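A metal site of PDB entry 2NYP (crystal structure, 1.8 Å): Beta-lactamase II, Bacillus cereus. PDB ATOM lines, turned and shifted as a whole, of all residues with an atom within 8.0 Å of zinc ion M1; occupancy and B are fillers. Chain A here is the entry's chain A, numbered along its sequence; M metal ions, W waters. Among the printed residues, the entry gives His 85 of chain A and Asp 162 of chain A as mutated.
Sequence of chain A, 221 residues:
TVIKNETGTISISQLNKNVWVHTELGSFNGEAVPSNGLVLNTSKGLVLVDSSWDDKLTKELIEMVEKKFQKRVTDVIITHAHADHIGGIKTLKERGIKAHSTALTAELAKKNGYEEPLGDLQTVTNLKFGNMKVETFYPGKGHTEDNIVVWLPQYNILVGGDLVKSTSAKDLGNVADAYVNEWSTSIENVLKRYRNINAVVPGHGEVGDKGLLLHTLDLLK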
ATOM      1  N   THR A  79      -7.818  34.259 -15.755  1.00  0.00           N
ATOM      2  CA  THR A  79      -8.340  33.044 -15.123  1.00  0.00           C
ATOM      3  C   THR A  79      -7.861  32.817 -13.683  1.00  0.00           C
ATOM      4  O   THR A  79      -8.428  32.027 -12.954  1.00  0.00           O
ATOM      5  CB  THR A  79      -8.108  31.799 -15.999  1.00  0.00           C
ATOM      6  OG1 THR A  79      -6.706  31.611 -16.154  1.00  0.00           O
ATOM      7  CG2 THR A  79      -8.814  31.956 -17.398  1.00  0.00           C
ATOM      8  N   HIS A  80      -6.793  33.504 -13.295  1.00  0.00           N
ATOM      9  CA  HIS A  80      -6.503  33.729 -11.891  1.00  0.00           C
ATOM     10  C   HIS A  80      -5.503  34.864 -11.673  1.00  0.00           C
ATOM     11  O   HIS A  80      -5.004  35.431 -12.621  1.00  0.00           O
ATOM     12  CB  HIS A  80      -6.129  32.444 -11.125  1.00  0.00           C
ATOM     13  CG  HIS A  80      -4.828  31.833 -11.527  1.00  0.00           C
ATOM     14  ND1 HIS A  80      -4.681  31.139 -12.708  1.00  0.00           N
ATOM     15  CD2 HIS A  80      -3.643  31.754 -10.884  1.00  0.00           C
ATOM     16  CE1 HIS A  80      -3.445  30.681 -12.781  1.00  0.00           C
ATOM     17  NE2 HIS A  80      -2.795  31.042 -11.696  1.00  0.00           N
ATOM     18  N   ALA A  81      -5.217  35.182 -10.400  1.00  0.00           N
ATOM     19  CA  ALA A  81      -4.549  36.431 -10.037  1.00  0.00           C
ATOM     20  C   ALA A  81      -3.038  36.262  -9.935  1.00  0.00           C
ATOM     21  O   ALA A  81      -2.331  37.189  -9.560  1.00  0.00           O
ATOM     22  CB  ALA A  81      -5.116  36.939  -8.720  1.00  0.00           C
ATOM     23  N   HIS A  82      -2.521  35.080 -10.246  1.00  0.00           N
ATOM     24  CA  HIS A  82      -1.078  34.917 -10.186  1.00  0.00           C
ATOM     25  C   HIS A  82      -0.371  35.850 -11.134  1.00  0.00           C
ATOM     26  O   HIS A  82      -0.865  36.149 -12.248  1.00  0.00           O
ATOM     27  CB  HIS A  82      -0.635  33.483 -10.440  1.00  0.00           C
ATOM     28  CG  HIS A  82      -0.536  32.659  -9.198  1.00  0.00           C
ATOM     29  ND1 HIS A  82      -0.495  31.281  -9.226  1.00  0.00           N
ATOM     30  CD2 HIS A  82      -0.481  33.022  -7.895  1.00  0.00           C
ATOM     31  CE1 HIS A  82      -0.397  30.834  -7.986  1.00  0.00           C
ATOM     32  NE2 HIS A  82      -0.387  31.854  -7.159  1.00  0.00           N
ATOM     33  N   ALA A  83       0.806  36.290 -10.688  1.00  0.00           N
ATOM     34  CA  ALA A  83       1.692  37.134 -11.505  1.00  0.00           C
ATOM     35  C   ALA A  83       1.674  36.799 -12.992  1.00  0.00           C
ATOM     36  O   ALA A  83       1.541  37.679 -13.811  1.00  0.00           O
ATOM     37  CB  ALA A  83       3.131  37.090 -10.973  1.00  0.00           C
ATOM     38  N   ASP A  84       1.783  35.530 -13.340  1.00  0.00           N
ATOM     39  CA  ASP A  84       1.865  35.121 -14.756  1.00  0.00           C
ATOM     40  C   ASP A  84       0.562  35.218 -15.562  1.00  0.00           C
ATOM     41  O   ASP A  84       0.571  35.040 -16.800  1.00  0.00           O
ATOM     42  CB  ASP A  84       2.473  33.711 -14.890  1.00  0.00           C
ATOM     43  CG  ASP A  84       1.657  32.621 -14.191  1.00  0.00           C
ATOM     44  OD1 ASP A  84       0.867  32.908 -13.253  1.00  0.00           O
ATOM     45  OD2 ASP A  84       1.794  31.451 -14.607  1.00  0.00           O
ATOM     46  N   HIS A  85      -0.530  35.513 -14.863  1.00  0.00           N
ATOM     47  CA  HIS A  85      -1.843  35.737 -15.486  1.00  0.00           C
ATOM     48  C   HIS A  85      -2.289  37.187 -15.399  1.00  0.00           C
ATOM     49  O   HIS A  85      -2.821  37.705 -16.354  1.00  0.00           O
ATOM     50  CB  HIS A  85      -2.882  34.827 -14.814  1.00  0.00           C
ATOM     51  CG  HIS A  85      -2.714  33.394 -15.181  1.00  0.00           C
ATOM     52  ND1 HIS A  85      -3.603  32.745 -15.994  1.00  0.00           N
ATOM     53  CD2 HIS A  85      -1.715  32.514 -14.924  1.00  0.00           C
ATOM     54  CE1 HIS A  85      -3.188  31.508 -16.208  1.00  0.00           C
ATOM     55  NE2 HIS A  85      -2.045  31.341 -15.561  1.00  0.00           N
ATOM     56  N   HIS A 143      -5.606  24.970  -8.170  1.00  0.00           N
ATOM     57  CA  HIS A 143      -4.280  25.511  -8.344  1.00  0.00           C
ATOM     58  C   HIS A 143      -4.124  26.788  -7.489  1.00  0.00           C
ATOM     59  O   HIS A 143      -3.108  27.000  -6.830  1.00  0.00           O
ATOM     60  CB  HIS A 143      -4.090  25.858  -9.812  1.00  0.00           C
ATOM     61  CG  HIS A 143      -2.896  26.706 -10.055  1.00  0.00           C
ATOM     62  ND1 HIS A 143      -1.625  26.203  -9.921  1.00  0.00           N
ATOM     63  CD2 HIS A 143      -2.756  28.014 -10.355  1.00  0.00           C
ATOM     64  CE1 HIS A 143      -0.744  27.162 -10.162  1.00  0.00           C
ATOM     65  NE2 HIS A 143      -1.405  28.266 -10.462  1.00  0.00           N
ATOM     66  N   THR A 144      -5.181  27.603  -7.493  1.00  0.00           N
ATOM     67  CA  THR A 144      -5.300  28.728  -6.564  1.00  0.00           C
ATOM     68  C   THR A 144      -6.721  28.771  -6.087  1.00  0.00           C
ATOM     69  O   THR A 144      -7.607  28.009  -6.558  1.00  0.00           O
ATOM     70  CB  THR A 144      -4.983  30.066  -7.258  1.00  0.00           C
ATOM     71  OG1 THR A 144      -5.844  30.217  -8.389  1.00  0.00           O
ATOM     72  CG2 THR A 144      -3.482  30.212  -7.631  1.00  0.00           C
ATOM     73  N   ASP A 146      -8.742  31.040  -6.652  1.00  0.00           N
ATOM     74  CA  ASP A 146      -9.598  31.842  -7.499  1.00  0.00           C
ATOM     75  C   ASP A 146      -9.725  31.306  -8.909  1.00  0.00           C
ATOM     76  O   ASP A 146     -10.501  31.845  -9.684  1.00  0.00           O
ATOM     77  CB  ASP A 146      -9.126  33.298  -7.583  1.00  0.00           C
ATOM     78  CG  ASP A 146      -7.692  33.454  -8.101  1.00  0.00           C
ATOM     79  OD1 ASP A 146      -6.822  32.677  -7.661  1.00  0.00           O
ATOM     80  OD2 ASP A 146      -7.448  34.353  -8.925  1.00  0.00           O
ATOM     81  N   ASN A 147      -8.947  30.259  -9.233  1.00  0.00           N
ATOM     82  CA  ASN A 147      -8.885  29.787 -10.617  1.00  0.00           C
ATOM     83  C   ASN A 147     -10.274  29.565 -11.243  1.00  0.00           C
ATOM     84  O   ASN A 147     -11.158  28.927 -10.640  1.00  0.00           O
ATOM     85  CB  ASN A 147      -8.012  28.517 -10.809  1.00  0.00           C
ATOM     86  CG  ASN A 147      -8.265  27.402  -9.778  1.00  0.00           C
ATOM     87  OD1 ASN A 147      -7.311  26.681  -9.446  1.00  0.00           O
ATOM     88  ND2 ASN A 147      -9.503  27.216  -9.292  1.00  0.00           N
ATOM     89  N   GLY A 161      -6.874  26.471 -17.814  1.00  0.00           N
ATOM     90  CA  GLY A 161      -5.856  27.266 -17.135  1.00  0.00           C
ATOM     91  C   GLY A 161      -5.016  26.359 -16.224  1.00  0.00           C
ATOM     92  O   GLY A 161      -4.835  25.153 -16.522  1.00  0.00           O
ATOM     93  N   ASP A 162      -4.520  26.889 -15.116  1.00  0.00           N
ATOM     94  CA  ASP A 162      -3.625  26.101 -14.272  1.00  0.00           C
ATOM     95  C   ASP A 162      -4.330  25.105 -13.397  1.00  0.00           C
ATOM     96  O   ASP A 162      -3.676  24.309 -12.756  1.00  0.00           O
ATOM     97  CB  ASP A 162      -2.704  26.957 -13.426  1.00  0.00           C
ATOM     98  CG  ASP A 162      -1.706  27.682 -14.271  1.00  0.00           C
ATOM     99  OD1 ASP A 162      -1.725  28.886 -14.186  1.00  0.00           O
ATOM    100  OD2 ASP A 162      -0.945  27.051 -15.020  1.00  0.00           O
ATOM    101  N   LEU A 163      -5.656  25.099 -13.422  1.00  0.00           N
ATOM    102  CA  LEU A 163      -6.432  24.071 -12.743  1.00  0.00           C
ATOM    103  C   LEU A 163      -6.121  22.727 -13.422  1.00  0.00           C
ATOM    104  O   LEU A 163      -6.213  21.678 -12.810  1.00  0.00           O
ATOM    105  CB  LEU A 163      -7.934  24.344 -12.852  1.00  0.00           C
ATOM    106  CG  LEU A 163      -8.901  23.448 -12.031  1.00  0.00           C
ATOM    107  CD1 LEU A 163      -8.801  23.728 -10.532  1.00  0.00           C
ATOM    108  CD2 LEU A 163     -10.313  23.716 -12.519  1.00  0.00           C
ATOM    109  N   LYS A 165      -3.643  20.250 -15.632  1.00  0.00           N
ATOM    110  CA  LYS A 165      -2.258  19.947 -16.022  1.00  0.00           C
ATOM    111  C   LYS A 165      -2.192  19.134 -17.322  1.00  0.00           C
ATOM    112  O   LYS A 165      -3.050  18.316 -17.593  1.00  0.00           O
ATOM    113  CB  LYS A 165      -1.532  19.224 -14.854  1.00  0.00           C
ATOM    114  CG  LYS A 165      -1.592  20.040 -13.517  1.00  0.00           C
ATOM    115  CD  LYS A 165      -0.742  21.325 -13.593  1.00  0.00           C
ATOM    116  CE  LYS A 165      -1.246  22.455 -12.644  1.00  0.00           C
ATOM    117  NZ  LYS A 165      -0.978  23.886 -13.199  1.00  0.00           N
ATOM    118  N   ASN A 174       3.588  24.578  -9.029  1.00  0.00           N
ATOM    119  CA  ASN A 174       3.589  25.440  -7.853  1.00  0.00           C
ATOM    120  C   ASN A 174       2.325  25.255  -6.989  1.00  0.00           C
ATOM    121  O   ASN A 174       1.230  25.637  -7.411  1.00  0.00           O
ATOM    122  CB  ASN A 174       3.749  26.894  -8.321  1.00  0.00           C
ATOM    123  CG  ASN A 174       3.572  27.894  -7.198  1.00  0.00           C
ATOM    124  OD1 ASN A 174       3.872  27.606  -6.040  1.00  0.00           O
ATOM    125  ND2 ASN A 174       3.053  29.080  -7.543  1.00  0.00           N
ATOM    126  N   ASP A 177       0.071  28.260  -3.387  1.00  0.00           N
ATOM    127  CA  ASP A 177      -1.249  28.890  -3.279  1.00  0.00           C
ATOM    128  C   ASP A 177      -2.404  27.956  -3.524  1.00  0.00           C
ATOM    129  O   ASP A 177      -3.517  28.396  -3.734  1.00  0.00           O
ATOM    130  CB  ASP A 177      -1.277  30.108  -4.220  1.00  0.00           C
ATOM    131  CG  ASP A 177      -0.236  31.147  -3.826  1.00  0.00           C
ATOM    132  OD1 ASP A 177       0.080  31.279  -2.632  1.00  0.00           O
ATOM    133  OD2 ASP A 177       0.278  31.804  -4.719  1.00  0.00           O
ATOM    134  N   HIS A 204      -0.465  25.161 -19.125  1.00  0.00           N
ATOM    135  CA  HIS A 204       0.833  24.967 -19.752  1.00  0.00           C
ATOM    136  C   HIS A 204       0.810  23.637 -20.419  1.00  0.00           C
ATOM    137  O   HIS A 204       0.285  22.662 -19.862  1.00  0.00           O
ATOM    138  CB  HIS A 204       1.962  24.953 -18.693  1.00  0.00           C
ATOM    139  CG  HIS A 204       1.926  26.119 -17.752  1.00  0.00           C
ATOM    140  ND1 HIS A 204       2.584  27.299 -18.007  1.00  0.00           N
ATOM    141  CD2 HIS A 204       1.289  26.275 -16.568  1.00  0.00           C
ATOM    142  CE1 HIS A 204       2.364  28.147 -17.012  1.00  0.00           C
ATOM    143  NE2 HIS A 204       1.569  27.558 -16.133  1.00  0.00           N
HETATM  144 ZN    ZN M   1      -0.962  30.226 -10.962  1.00  0.00          ZN
HETATM  145 ZN    ZN M   2      -0.550  29.959 -15.664  1.00  0.00          ZN
HETATM  146  O   HOH W   1       1.372  29.275 -10.611  1.00  0.00           O
HETATM  147  O   HOH W   2       0.249  30.024 -13.343  1.00  0.00           O
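N of His 143 sits at hydrogen-bond distance from OD1 of Asn 147 (2.7 Å).
NE2 of His 82 sits at hydrogen-bond distance from OD2 of Asp 177, 2.5 Å away.
A ring nitrogen (NE2) of His 204 lies within hydrogen-bond range of the side-chain carboxylate of Asp 162 (2.8 Å).
NZ of Lys 165 is in salt-bridge range of OD2 of Asp 162 (3.7 Å).
Residues that only touch zinc ion M1: Asp 84 (3.97 Å) and Asp 162 (3.6 Å).
A ring nitrogen (NE2) of His 143 is bound to zinc ion M1 (2.1 Å).
Zinc ion M1 is bound by a ring nitrogen (ND1) of His 82.
NE2 of His 80 binds zinc ion M1, at 2.1 Å.
Water W1 is bound to zinc ion M1 (2.5 Å).
Slightly farther from zinc ion M1 lies water W2 (2.7 Å).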
